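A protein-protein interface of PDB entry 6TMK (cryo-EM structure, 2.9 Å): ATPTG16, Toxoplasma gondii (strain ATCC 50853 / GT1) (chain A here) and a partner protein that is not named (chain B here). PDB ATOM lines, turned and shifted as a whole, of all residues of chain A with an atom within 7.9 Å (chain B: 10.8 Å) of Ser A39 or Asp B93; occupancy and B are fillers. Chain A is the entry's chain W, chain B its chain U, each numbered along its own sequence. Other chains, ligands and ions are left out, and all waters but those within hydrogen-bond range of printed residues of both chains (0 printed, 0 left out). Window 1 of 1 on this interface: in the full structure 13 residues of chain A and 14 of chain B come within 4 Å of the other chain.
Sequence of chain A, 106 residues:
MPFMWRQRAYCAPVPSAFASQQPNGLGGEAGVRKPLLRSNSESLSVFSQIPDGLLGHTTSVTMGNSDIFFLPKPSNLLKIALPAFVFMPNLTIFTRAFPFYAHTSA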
ATOM      1  N   TRP A   5      -2.679  11.235 -22.792  1.00  0.00           N
ATOM      2  CA  TRP A   5      -3.704  10.594 -21.984  1.00  0.00           C
ATOM      3  C   TRP A   5      -5.022  11.350 -22.045  1.00  0.00           C
ATOM      4  O   TRP A   5      -6.086  10.738 -22.178  1.00  0.00           O
ATOM      5  CB  TRP A   5      -3.221  10.475 -20.546  1.00  0.00           C
ATOM      6  CG  TRP A   5      -2.058   9.556 -20.373  1.00  0.00           C
ATOM      7  CD1 TRP A   5      -0.800   9.903 -19.996  1.00  0.00           C
ATOM      8  CD2 TRP A   5      -2.037   8.139 -20.575  1.00  0.00           C
ATOM      9  NE1 TRP A   5       0.002   8.799 -19.945  1.00  0.00           N
ATOM     10  CE2 TRP A   5      -0.733   7.702 -20.297  1.00  0.00           C
ATOM     11  CE3 TRP A   5      -2.991   7.200 -20.964  1.00  0.00           C
ATOM     12  CZ2 TRP A   5      -0.362   6.371 -20.388  1.00  0.00           C
ATOM     13  CZ3 TRP A   5      -2.618   5.883 -21.056  1.00  0.00           C
ATOM     14  CH2 TRP A   5      -1.320   5.478 -20.769  1.00  0.00           C
ATOM     15  N   ALA A   9      -9.052   9.149 -25.187  1.00  0.00           N
ATOM     16  CA  ALA A   9     -10.069   8.711 -24.246  1.00  0.00           C
ATOM     17  C   ALA A   9     -10.430   7.247 -24.414  1.00  0.00           C
ATOM     18  O   ALA A   9     -10.917   6.626 -23.464  1.00  0.00           O
ATOM     19  CB  ALA A   9     -11.313   9.574 -24.395  1.00  0.00           C
ATOM     20  N   TYR A  10     -10.215   6.687 -25.603  1.00  0.00           N
ATOM     21  CA  TYR A  10     -10.506   5.278 -25.823  1.00  0.00           C
ATOM     22  C   TYR A  10      -9.646   4.376 -24.948  1.00  0.00           C
ATOM     23  O   TYR A  10     -10.082   3.281 -24.576  1.00  0.00           O
ATOM     24  CB  TYR A  10     -10.335   4.928 -27.299  1.00  0.00           C
ATOM     25  CG  TYR A  10      -9.093   5.470 -27.958  1.00  0.00           C
ATOM     26  CD1 TYR A  10      -7.857   4.915 -27.712  1.00  0.00           C
ATOM     27  CD2 TYR A  10      -9.165   6.535 -28.832  1.00  0.00           C
ATOM     28  CE1 TYR A  10      -6.733   5.408 -28.308  1.00  0.00           C
ATOM     29  CE2 TYR A  10      -8.045   7.030 -29.435  1.00  0.00           C
ATOM     30  CZ  TYR A  10      -6.828   6.459 -29.174  1.00  0.00           C
ATOM     31  OH  TYR A  10      -5.699   6.951 -29.773  1.00  0.00           O
ATOM     32  N   CYS A  11      -8.433   4.804 -24.609  1.00  0.00           N
ATOM     33  CA  CYS A  11      -7.520   3.998 -23.813  1.00  0.00           C
ATOM     34  C   CYS A  11      -7.574   4.363 -22.333  1.00  0.00           C
ATOM     35  O   CYS A  11      -6.630   4.073 -21.592  1.00  0.00           O
ATOM     36  CB  CYS A  11      -6.091   4.141 -24.334  1.00  0.00           C
ATOM     37  SG  CYS A  11      -5.331   5.726 -24.006  1.00  0.00           S
ATOM     38  N   ALA A  12      -8.655   4.980 -21.895  1.00  0.00           N
ATOM     39  CA  ALA A  12      -8.783   5.525 -20.560  1.00  0.00           C
ATOM     40  C   ALA A  12      -9.703   4.664 -19.710  1.00  0.00           C
ATOM     41  O   ALA A  12     -10.499   3.879 -20.234  1.00  0.00           O
ATOM     42  CB  ALA A  12      -9.331   6.953 -20.609  1.00  0.00           C
ATOM     43  N   PRO A  13      -9.623   4.781 -18.390  1.00  0.00           N
ATOM     44  CA  PRO A  13     -10.515   3.998 -17.540  1.00  0.00           C
ATOM     45  C   PRO A  13     -11.943   4.503 -17.622  1.00  0.00           C
ATOM     46  O   PRO A  13     -12.222   5.639 -18.009  1.00  0.00           O
ATOM     47  CB  PRO A  13      -9.938   4.183 -16.135  1.00  0.00           C
ATOM     48  CG  PRO A  13      -9.094   5.349 -16.205  1.00  0.00           C
ATOM     49  CD  PRO A  13      -8.647   5.544 -17.602  1.00  0.00           C
ATOM     50  N   VAL A  14     -12.857   3.621 -17.245  1.00  0.00           N
ATOM     51  CA  VAL A  14     -14.277   3.930 -17.262  1.00  0.00           C
ATOM     52  C   VAL A  14     -14.593   4.847 -16.089  1.00  0.00           C
ATOM     53  O   VAL A  14     -13.834   4.890 -15.113  1.00  0.00           O
ATOM     54  CB  VAL A  14     -15.120   2.647 -17.228  1.00  0.00           C
ATOM     55  CG1 VAL A  14     -14.727   1.750 -18.369  1.00  0.00           C
ATOM     56  CG2 VAL A  14     -14.952   1.924 -15.914  1.00  0.00           C
ATOM     57  N   PRO A  15     -15.684   5.607 -16.147  1.00  0.00           N
ATOM     58  CA  PRO A  15     -15.999   6.521 -15.043  1.00  0.00           C
ATOM     59  C   PRO A  15     -16.307   5.828 -13.734  1.00  0.00           C
ATOM     60  O   PRO A  15     -16.262   6.479 -12.684  1.00  0.00           O
ATOM     61  CB  PRO A  15     -17.211   7.301 -15.572  1.00  0.00           C
ATOM     62  CG  PRO A  15     -17.694   6.547 -16.735  1.00  0.00           C
ATOM     63  CD  PRO A  15     -16.531   5.858 -17.318  1.00  0.00           C
ATOM     64  N   ALA A  17     -14.365   3.809 -12.446  1.00  0.00           N
ATOM     65  CA  ALA A  17     -13.064   3.613 -11.832  1.00  0.00           C
ATOM     66  C   ALA A  17     -12.626   4.808 -10.999  1.00  0.00           C
ATOM     67  O   ALA A  17     -11.903   4.635 -10.013  1.00  0.00           O
ATOM     68  CB  ALA A  17     -12.032   3.324 -12.914  1.00  0.00           C
ATOM     69  N   LEU A  36     -11.845  -3.740 -10.238  1.00  0.00           N
ATOM     70  CA  LEU A  36     -12.065  -2.328  -9.958  1.00  0.00           C
ATOM     71  C   LEU A  36     -11.696  -1.436 -11.129  1.00  0.00           C
ATOM     72  O   LEU A  36     -12.343  -0.407 -11.348  1.00  0.00           O
ATOM     73  CB  LEU A  36     -11.264  -1.911  -8.727  1.00  0.00           C
ATOM     74  CG  LEU A  36     -11.432  -2.790  -7.495  1.00  0.00           C
ATOM     75  CD1 LEU A  36     -10.480  -2.349  -6.422  1.00  0.00           C
ATOM     76  CD2 LEU A  36     -12.850  -2.748  -6.997  1.00  0.00           C
ATOM     77  N   LEU A  37     -10.667  -1.811 -11.875  1.00  0.00           N
ATOM     78  CA  LEU A  37     -10.155  -1.031 -12.988  1.00  0.00           C
ATOM     79  C   LEU A  37     -10.542  -1.688 -14.302  1.00  0.00           C
ATOM     80  O   LEU A  37     -10.277  -2.876 -14.509  1.00  0.00           O
ATOM     81  CB  LEU A  37      -8.639  -0.900 -12.882  1.00  0.00           C
ATOM     82  CG  LEU A  37      -7.920   0.099 -13.770  1.00  0.00           C
ATOM     83  CD1 LEU A  37      -8.470   1.480 -13.580  1.00  0.00           C
ATOM     84  CD2 LEU A  37      -6.459   0.066 -13.407  1.00  0.00           C
ATOM     85  N   ARG A  38     -11.166  -0.914 -15.184  1.00  0.00           N
ATOM     86  CA  ARG A  38     -11.480  -1.361 -16.530  1.00  0.00           C
ATOM     87  C   ARG A  38     -11.275  -0.203 -17.491  1.00  0.00           C
ATOM     88  O   ARG A  38     -11.457   0.963 -17.132  1.00  0.00           O
ATOM     89  CB  ARG A  38     -12.911  -1.891 -16.638  1.00  0.00           C
ATOM     90  CG  ARG A  38     -13.214  -2.995 -15.660  1.00  0.00           C
ATOM     91  CD  ARG A  38     -14.541  -3.657 -15.946  1.00  0.00           C
ATOM     92  NE  ARG A  38     -15.643  -2.702 -15.902  1.00  0.00           N
ATOM     93  CZ  ARG A  38     -16.204  -2.147 -16.971  1.00  0.00           C
ATOM     94  NH1 ARG A  38     -15.783  -2.438 -18.192  1.00  0.00           N
ATOM     95  NH2 ARG A  38     -17.193  -1.288 -16.813  1.00  0.00           N
ATOM     96  N   SER A  39     -10.878  -0.535 -18.710  1.00  0.00           N
ATOM     97  CA  SER A  39     -10.610   0.450 -19.741  1.00  0.00           C
ATOM     98  C   SER A  39     -11.793   0.576 -20.690  1.00  0.00           C
ATOM     99  O   SER A  39     -12.674  -0.284 -20.746  1.00  0.00           O
ATOM    100  CB  SER A  39      -9.361   0.056 -20.525  1.00  0.00           C
ATOM    101  OG  SER A  39      -9.013   1.015 -21.496  1.00  0.00           O
ATOM    102  N   ASN A  40     -11.800   1.675 -21.439  1.00  0.00           N
ATOM    103  CA  ASN A  40     -12.738   1.835 -22.539  1.00  0.00           C
ATOM    104  C   ASN A  40     -12.289   1.101 -23.793  1.00  0.00           C
ATOM    105  O   ASN A  40     -13.100   0.897 -24.700  1.00  0.00           O
ATOM    106  CB  ASN A  40     -12.933   3.317 -22.845  1.00  0.00           C
ATOM    107  CG  ASN A  40     -13.902   3.981 -21.904  1.00  0.00           C
ATOM    108  OD1 ASN A  40     -14.963   3.441 -21.602  1.00  0.00           O
ATOM    109  ND2 ASN A  40     -13.545   5.163 -21.434  1.00  0.00           N
ATOM    110  N   SER A  41     -11.021   0.698 -23.858  1.00  0.00           N
ATOM    111  CA  SER A  41     -10.504  -0.058 -24.986  1.00  0.00           C
ATOM    112  C   SER A  41     -11.067  -1.466 -25.043  1.00  0.00           C
ATOM    113  O   SER A  41     -10.911  -2.141 -26.066  1.00  0.00           O
ATOM    114  CB  SER A  41      -8.982  -0.106 -24.909  1.00  0.00           C
ATOM    115  OG  SER A  41      -8.554  -0.758 -23.735  1.00  0.00           O
ATOM    116  N   GLU A  42     -11.711  -1.921 -23.973  1.00  0.00           N
ATOM    117  CA  GLU A  42     -12.399  -3.198 -23.993  1.00  0.00           C
ATOM    118  C   GLU A  42     -13.631  -3.173 -24.882  1.00  0.00           C
ATOM    119  O   GLU A  42     -14.138  -4.236 -25.249  1.00  0.00           O
ATOM    120  CB  GLU A  42     -12.804  -3.552 -22.572  1.00  0.00           C
ATOM    121  CG  GLU A  42     -11.683  -4.104 -21.736  1.00  0.00           C
ATOM    122  CD  GLU A  42     -12.175  -4.777 -20.477  1.00  0.00           C
ATOM    123  OE1 GLU A  42     -13.395  -4.730 -20.212  1.00  0.00           O
ATOM    124  OE2 GLU A  42     -11.340  -5.347 -19.745  1.00  0.00           O
ATOM    125  N   SER A  43     -14.116  -1.984 -25.238  1.00  0.00           N
ATOM    126  CA  SER A  43     -15.219  -1.873 -26.179  1.00  0.00           C
ATOM    127  C   SER A  43     -14.843  -2.375 -27.563  1.00  0.00           C
ATOM    128  O   SER A  43     -15.730  -2.692 -28.360  1.00  0.00           O
ATOM    129  CB  SER A  43     -15.671  -0.418 -26.260  1.00  0.00           C
ATOM    130  OG  SER A  43     -16.154   0.025 -25.010  1.00  0.00           O
ATOM    131  N   LEU A  44     -13.550  -2.456 -27.861  1.00  0.00           N
ATOM    132  CA  LEU A  44     -13.080  -2.942 -29.148  1.00  0.00           C
ATOM    133  C   LEU A  44     -12.995  -4.456 -29.222  1.00  0.00           C
ATOM    134  O   LEU A  44     -12.553  -4.983 -30.247  1.00  0.00           O
ATOM    135  CB  LEU A  44     -11.723  -2.332 -29.477  1.00  0.00           C
ATOM    136  CG  LEU A  44     -11.685  -0.810 -29.472  1.00  0.00           C
ATOM    137  CD1 LEU A  44     -10.277  -0.337 -29.613  1.00  0.00           C
ATOM    138  CD2 LEU A  44     -12.539  -0.260 -30.581  1.00  0.00           C
ATOM    139  N   SER A  45     -13.382  -5.162 -28.169  1.00  0.00           N
ATOM    140  CA  SER A  45     -13.427  -6.610 -28.178  1.00  0.00           C
ATOM    141  C   SER A  45     -14.867  -7.064 -28.012  1.00  0.00           C
ATOM    142  O   SER A  45     -15.657  -6.437 -27.302  1.00  0.00           O
ATOM    143  CB  SER A  45     -12.558  -7.203 -27.069  1.00  0.00           C
ATOM    144  OG  SER A  45     -11.189  -6.931 -27.295  1.00  0.00           O
ATOM    145  N   SER A  48     -15.193  -9.592 -24.533  1.00  0.00           N
ATOM    146  CA  SER A  48     -14.599  -9.072 -23.310  1.00  0.00           C
ATOM    147  C   SER A  48     -15.492  -9.338 -22.106  1.00  0.00           C
ATOM    148  O   SER A  48     -15.112 -10.056 -21.176  1.00  0.00           O
ATOM    149  CB  SER A  48     -14.337  -7.575 -23.458  1.00  0.00           C
ATOM    150  OG  SER A  48     -15.555  -6.866 -23.553  1.00  0.00           O
ATOM    151  N   LYS B  84      -6.615 -17.518 -24.237  1.00  0.00           N
ATOM    152  CA  LYS B  84      -5.330 -16.854 -24.051  1.00  0.00           C
ATOM    153  C   LYS B  84      -5.351 -15.447 -24.634  1.00  0.00           C
ATOM    154  O   LYS B  84      -4.896 -14.485 -24.001  1.00  0.00           O
ATOM    155  CB  LYS B  84      -4.228 -17.689 -24.689  1.00  0.00           C
ATOM    156  CG  LYS B  84      -3.922 -18.937 -23.946  1.00  0.00           C
ATOM    157  CD  LYS B  84      -2.894 -19.767 -24.653  1.00  0.00           C
ATOM    158  CE  LYS B  84      -2.694 -21.093 -23.954  1.00  0.00           C
ATOM    159  NZ  LYS B  84      -3.531 -22.172 -24.546  1.00  0.00           N
ATOM    160  N   GLN B  85      -5.883 -15.314 -25.847  1.00  0.00           N
ATOM    161  CA  GLN B  85      -5.962 -14.018 -26.510  1.00  0.00           C
ATOM    162  C   GLN B  85      -6.793 -13.033 -25.697  1.00  0.00           C
ATOM    163  O   GLN B  85      -6.408 -11.869 -25.508  1.00  0.00           O
ATOM    164  CB  GLN B  85      -6.548 -14.228 -27.898  1.00  0.00           C
ATOM    165  CG  GLN B  85      -6.772 -13.006 -28.703  1.00  0.00           C
ATOM    166  CD  GLN B  85      -7.171 -13.339 -30.111  1.00  0.00           C
ATOM    167  OE1 GLN B  85      -7.343 -14.503 -30.459  1.00  0.00           O
ATOM    168  NE2 GLN B  85      -7.326 -12.327 -30.928  1.00  0.00           N
ATOM    169  N   LYS B  86      -7.946 -13.490 -25.218  1.00  0.00           N
ATOM    170  CA  LYS B  86      -8.831 -12.661 -24.417  1.00  0.00           C
ATOM    171  C   LYS B  86      -8.119 -12.132 -23.186  1.00  0.00           C
ATOM    172  O   LYS B  86      -8.183 -10.936 -22.879  1.00  0.00           O
ATOM    173  CB  LYS B  86     -10.046 -13.487 -24.012  1.00  0.00           C
ATOM    174  CG  LYS B  86     -11.174 -12.712 -23.405  1.00  0.00           C
ATOM    175  CD  LYS B  86     -12.004 -13.586 -22.505  1.00  0.00           C
ATOM    176  CE  LYS B  86     -12.850 -14.552 -23.293  1.00  0.00           C
ATOM    177  NZ  LYS B  86     -13.148 -15.760 -22.489  1.00  0.00           N
ATOM    178  N   LEU B  87      -7.449 -13.019 -22.454  1.00  0.00           N
ATOM    179  CA  LEU B  87      -6.819 -12.598 -21.211  1.00  0.00           C
ATOM    180  C   LEU B  87      -5.652 -11.659 -21.476  1.00  0.00           C
ATOM    181  O   LEU B  87      -5.427 -10.709 -20.714  1.00  0.00           O
ATOM    182  CB  LEU B  87      -6.376 -13.823 -20.423  1.00  0.00           C
ATOM    183  CG  LEU B  87      -7.488 -14.798 -20.057  1.00  0.00           C
ATOM    184  CD1 LEU B  87      -6.949 -15.839 -19.130  1.00  0.00           C
ATOM    185  CD2 LEU B  87      -8.676 -14.108 -19.439  1.00  0.00           C
ATOM    186  N   PHE B  88      -4.917 -11.884 -22.565  1.00  0.00           N
ATOM    187  CA  PHE B  88      -3.868 -10.949 -22.944  1.00  0.00           C
ATOM    188  C   PHE B  88      -4.429  -9.551 -23.166  1.00  0.00           C
ATOM    189  O   PHE B  88      -3.921  -8.566 -22.616  1.00  0.00           O
ATOM    190  CB  PHE B  88      -3.164 -11.436 -24.206  1.00  0.00           C
ATOM    191  CG  PHE B  88      -2.126 -10.491 -24.705  1.00  0.00           C
ATOM    192  CD1 PHE B  88      -0.840 -10.547 -24.231  1.00  0.00           C
ATOM    193  CD2 PHE B  88      -2.446  -9.525 -25.633  1.00  0.00           C
ATOM    194  CE1 PHE B  88       0.104  -9.669 -24.681  1.00  0.00           C
ATOM    195  CE2 PHE B  88      -1.507  -8.650 -26.077  1.00  0.00           C
ATOM    196  CZ  PHE B  88      -0.233  -8.716 -25.598  1.00  0.00           C
ATOM    197  N   HIS B  89      -5.467  -9.446 -23.998  1.00  0.00           N
ATOM    198  CA  HIS B  89      -6.046  -8.140 -24.294  1.00  0.00           C
ATOM    199  C   HIS B  89      -6.585  -7.471 -23.038  1.00  0.00           C
ATOM    200  O   HIS B  89      -6.431  -6.256 -22.850  1.00  0.00           O
ATOM    201  CB  HIS B  89      -7.146  -8.297 -25.336  1.00  0.00           C
ATOM    202  CG  HIS B  89      -6.642  -8.370 -26.739  1.00  0.00           C
ATOM    203  ND1 HIS B  89      -7.165  -9.237 -27.672  1.00  0.00           N
ATOM    204  CD2 HIS B  89      -5.687  -7.658 -27.381  1.00  0.00           C
ATOM    205  CE1 HIS B  89      -6.536  -9.075 -28.820  1.00  0.00           C
ATOM    206  NE2 HIS B  89      -5.636  -8.121 -28.671  1.00  0.00           N
ATOM    207  N   GLN B  90      -7.212  -8.253 -22.166  1.00  0.00           N
ATOM    208  CA  GLN B  90      -7.716  -7.729 -20.906  1.00  0.00           C
ATOM    209  C   GLN B  90      -6.597  -7.103 -20.083  1.00  0.00           C
ATOM    210  O   GLN B  90      -6.694  -5.946 -19.648  1.00  0.00           O
ATOM    211  CB  GLN B  90      -8.392  -8.865 -20.150  1.00  0.00           C
ATOM    212  CG  GLN B  90      -9.416  -8.466 -19.152  1.00  0.00           C
ATOM    213  CD  GLN B  90     -10.279  -9.631 -18.744  1.00  0.00           C
ATOM    214  OE1 GLN B  90     -10.876 -10.298 -19.587  1.00  0.00           O
ATOM    215  NE2 GLN B  90     -10.322  -9.908 -17.450  1.00  0.00           N
ATOM    216  N   GLU B  91      -5.528  -7.865 -19.846  1.00  0.00           N
ATOM    217  CA  GLU B  91      -4.417  -7.367 -19.047  1.00  0.00           C
ATOM    218  C   GLU B  91      -3.806  -6.114 -19.661  1.00  0.00           C
ATOM    219  O   GLU B  91      -3.447  -5.169 -18.946  1.00  0.00           O
ATOM    220  CB  GLU B  91      -3.374  -8.467 -18.895  1.00  0.00           C
ATOM    221  CG  GLU B  91      -3.829  -9.607 -18.009  1.00  0.00           C
ATOM    222  CD  GLU B  91      -3.222 -10.937 -18.399  1.00  0.00           C
ATOM    223  OE1 GLU B  91      -2.167 -10.943 -19.067  1.00  0.00           O
ATOM    224  OE2 GLU B  91      -3.804 -11.981 -18.041  1.00  0.00           O
ATOM    225  N   LEU B  92      -3.677  -6.091 -20.988  1.00  0.00           N
ATOM    226  CA  LEU B  92      -3.098  -4.934 -21.664  1.00  0.00           C
ATOM    227  C   LEU B  92      -3.940  -3.683 -21.444  1.00  0.00           C
ATOM    228  O   LEU B  92      -3.414  -2.606 -21.121  1.00  0.00           O
ATOM    229  CB  LEU B  92      -2.967  -5.239 -23.151  1.00  0.00           C
ATOM    230  CG  LEU B  92      -2.273  -4.212 -24.033  1.00  0.00           C
ATOM    231  CD1 LEU B  92      -0.791  -4.425 -24.009  1.00  0.00           C
ATOM    232  CD2 LEU B  92      -2.796  -4.305 -25.443  1.00  0.00           C
ATOM    233  N   ASP B  93      -5.253  -3.805 -21.630  1.00  0.00           N
ATOM    234  CA  ASP B  93      -6.137  -2.666 -21.425  1.00  0.00           C
ATOM    235  C   ASP B  93      -6.057  -2.171 -19.988  1.00  0.00           C
ATOM    236  O   ASP B  93      -6.052  -0.957 -19.733  1.00  0.00           O
ATOM    237  CB  ASP B  93      -7.567  -3.052 -21.798  1.00  0.00           C
ATOM    238  CG  ASP B  93      -7.683  -3.529 -23.224  1.00  0.00           C
ATOM    239  OD1 ASP B  93      -6.987  -2.970 -24.099  1.00  0.00           O
ATOM    240  OD2 ASP B  93      -8.476  -4.459 -23.478  1.00  0.00           O
ATOM    241  N   ARG B  94      -5.997  -3.101 -19.036  1.00  0.00           N
ATOM    242  CA  ARG B  94      -5.883  -2.716 -17.636  1.00  0.00           C
ATOM    243  C   ARG B  94      -4.601  -1.938 -17.382  1.00  0.00           C
ATOM    244  O   ARG B  94      -4.611  -0.924 -16.674  1.00  0.00           O
ATOM    245  CB  ARG B  94      -5.894  -3.955 -16.752  1.00  0.00           C
ATOM    246  CG  ARG B  94      -7.064  -4.876 -16.926  1.00  0.00           C
ATOM    247  CD  ARG B  94      -8.126  -4.675 -15.909  1.00  0.00           C
ATOM    248  NE  ARG B  94      -9.207  -5.638 -16.087  1.00  0.00           N
ATOM    249  CZ  ARG B  94     -10.117  -5.564 -17.047  1.00  0.00           C
ATOM    250  NH1 ARG B  94     -11.062  -6.484 -17.131  1.00  0.00           N
ATOM    251  NH2 ARG B  94     -10.064  -4.589 -17.939  1.00  0.00           N
ATOM    252  N   GLU B  95      -3.486  -2.396 -17.955  1.00  0.00           N
ATOM    253  CA  GLU B  95      -2.221  -1.686 -17.799  1.00  0.00           C
ATOM    254  C   GLU B  95      -2.302  -0.271 -18.355  1.00  0.00           C
ATOM    255  O   GLU B  95      -1.792   0.678 -17.748  1.00  0.00           O
ATOM    256  CB  GLU B  95      -1.104  -2.469 -18.486  1.00  0.00           C
ATOM    257  CG  GLU B  95      -0.715  -3.739 -17.764  1.00  0.00           C
ATOM    258  CD  GLU B  95       0.008  -4.731 -18.662  1.00  0.00           C
ATOM    259  OE1 GLU B  95       0.464  -4.332 -19.754  1.00  0.00           O
ATOM    260  OE2 GLU B  95       0.119  -5.914 -18.275  1.00  0.00           O
ATOM    261  N   LEU B  96      -2.925  -0.112 -19.519  1.00  0.00           N
ATOM    262  CA  LEU B  96      -3.035   1.217 -20.114  1.00  0.00           C
ATOM    263  C   LEU B  96      -3.864   2.154 -19.239  1.00  0.00           C
ATOM    264  O   LEU B  96      -3.490   3.314 -19.015  1.00  0.00           O
ATOM    265  CB  LEU B  96      -3.622   1.106 -21.517  1.00  0.00           C
ATOM    266  CG  LEU B  96      -2.588   1.068 -22.640  1.00  0.00           C
ATOM    267  CD1 LEU B  96      -1.707  -0.171 -22.579  1.00  0.00           C
ATOM    268  CD2 LEU B  96      -3.325   1.116 -23.936  1.00  0.00           C
ATOM    269  N   ALA B  97      -5.001   1.670 -18.736  1.00  0.00           N
ATOM    270  CA  ALA B  97      -5.811   2.490 -17.837  1.00  0.00           C
ATOM    271  C   ALA B  97      -5.044   2.845 -16.566  1.00  0.00           C
ATOM    272  O   ALA B  97      -5.150   3.967 -16.051  1.00  0.00           O
ATOM    273  CB  ALA B  97      -7.115   1.770 -17.508  1.00  0.00           C
ATOM    274  N   ALA B  98      -4.257   1.901 -16.053  1.00  0.00           N
ATOM    275  CA  ALA B  98      -3.444   2.164 -14.873  1.00  0.00           C
ATOM    276  C   ALA B  98      -2.417   3.252 -15.143  1.00  0.00           C
ATOM    277  O   ALA B  98      -2.145   4.086 -14.277  1.00  0.00           O
ATOM    278  CB  ALA B  98      -2.754   0.883 -14.422  1.00  0.00           C
ATOM    279  N   GLY B  99      -1.840   3.262 -16.343  1.00  0.00           N
ATOM    280  CA  GLY B  99      -0.918   4.329 -16.701  1.00  0.00           C
ATOM    281  C   GLY B  99      -1.609   5.673 -16.793  1.00  0.00           C
ATOM    282  O   GLY B  99      -1.059   6.704 -16.383  1.00  0.00           O
ATOM    283  N   HIS B 100      -2.825   5.681 -17.327  1.00  0.00           N
ATOM    284  CA  HIS B 100      -3.605   6.910 -17.329  1.00  0.00           C
ATOM    285  C   HIS B 100      -3.787   7.442 -15.916  1.00  0.00           C
ATOM    286  O   HIS B 100      -3.641   8.644 -15.675  1.00  0.00           O
ATOM    287  CB  HIS B 100      -4.966   6.669 -17.969  1.00  0.00           C
ATOM    288  CG  HIS B 100      -5.772   7.914 -18.146  1.00  0.00           C
ATOM    289  ND1 HIS B 100      -6.263   8.635 -17.080  1.00  0.00           N
ATOM    290  CD2 HIS B 100      -6.192   8.556 -19.260  1.00  0.00           C
ATOM    291  CE1 HIS B 100      -6.933   9.679 -17.530  1.00  0.00           C
ATOM    292  NE2 HIS B 100      -6.907   9.653 -18.849  1.00  0.00           N
ATOM    293  N   ILE B 101      -4.106   6.564 -14.966  1.00  0.00           N
ATOM    294  CA  ILE B 101      -4.275   7.028 -13.593  1.00  0.00           C
ATOM    295  C   ILE B 101      -2.941   7.444 -12.987  1.00  0.00           C
ATOM    296  O   ILE B 101      -2.885   8.365 -12.166  1.00  0.00           O
ATOM    297  CB  ILE B 101      -4.968   5.961 -12.731  1.00  0.00           C
ATOM    298  CG1 ILE B 101      -6.421   5.805 -13.148  1.00  0.00           C
ATOM    299  CG2 ILE B 101      -4.871   6.321 -11.271  1.00  0.00           C
ATOM    300  CD1 ILE B 101      -7.037   4.546 -12.680  1.00  0.00           C
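Among the printed residues, pairs that only touch across the chains: Trp A5 with Leu B96 (3.4 Å), Leu A37 with Ile B101 (3.5 Å), Ser A39 with Asp B93 (3.6 Å), Trp A5 with His B100 (3.6 Å), Glu A42 with Asp B93 (3.7 Å), Glu A42 with Gln B90 (3.7 Å), Pro A13 with His B100 (3.8 Å), Ala A12 with His B100 (3.8 Å), Arg A38 with Arg B94 (3.8 Å), Trp A5 with Gly B99 (3.9 Å), Leu A37 with Ala B98 (3.9 Å) and Pro A13 with Ala B97 (3.96 Å).
Hydrophobic or aromatic side chains of chain A within 4 Å of the printed part of chain B: Trp A5, Ala A12, Pro A13 and Leu A37. Of the 18 printed residues of chain B, 9 touch a printed residue of chain A. Printed residues of chain B that touch a printed residue of chain A: Gln B90, Asp B93, Arg B94, Leu B96, Ala B97, Ala B98, Gly B99, His B100 and Ile B101. Hydrophobic or aromatic side chains of chain B within 4 Å of the printed part of chain A: Ala B97, Ala B98, His B100 and Ile B101. Among the printed residues, 15 pairs touch across the chains.
The backbone carbonyl oxygen (O) of Leu A37 sits close to the guanidinium group (NE) of Arg B94 (3.4 Å). OD1 of Asp B93 is in hydrogen-bond range of OG of Ser A41. OE2 of Glu A42 is in salt-bridge range of NH1 of Arg B94, 2.9 Å away.
Cys A11 touches none of the printed residues of chain B. Of chain B, only His B100 comes within 4 Å of Ala A12. Pro A13 touches just these residues of chain B: Ala B97 and His B100. Of the printed residues of chain B, Arg A38 touches Arg B94. Ser A39 touches just one residue of chain B: Asp B93 (3.6 Å). No residue of chain B comes within 4 Å of Asn A40. Of chain B, only Asp B93 comes within 4 Å of Ser A41. Of the printed residues of chain B, Glu A42 touches Gln B90 (3.7 Å), Asp B93 (3.7 Å) and Arg B94 (2.3 Å). Ser A43 touches none of the printed residues of chain B. Of the printed residues of chain A, Ala B98 touches Leu A37 (3.9 Å). Of the printed residues of chain A, His B100 touches Trp A5, Ala A12 and Pro A13. Printed residues of chain A within 4 Å of Ile B101: Leu A37 (3.5 Å). The nearest printed residue of chain A that does not touch Ile B101 is Pro A13 (4.1 Å).
The backbone carbonyl oxygen (O) of Tyr A10 lies within hydrogen-bond range of the backbone NH (N) of Ser A41 (2.8 Å). O of Ala A12 lies within hydrogen-bond range of OG of Ser A39 (3.5 Å). N of Val A14 is in hydrogen-bond range of O of Arg A38, at 3.0 Å. The guanidinium group of Arg A38 is in salt-bridge range of the side-chain carboxylate of Glu A42, at 3.9 Å. The side-chain hydroxyl (OG) of Ser A39 sits at hydrogen-bond distance from the side-chain hydroxyl (OG) of Ser A41. O of Glu A42 lies within hydrogen-bond range of OG of Ser A48.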
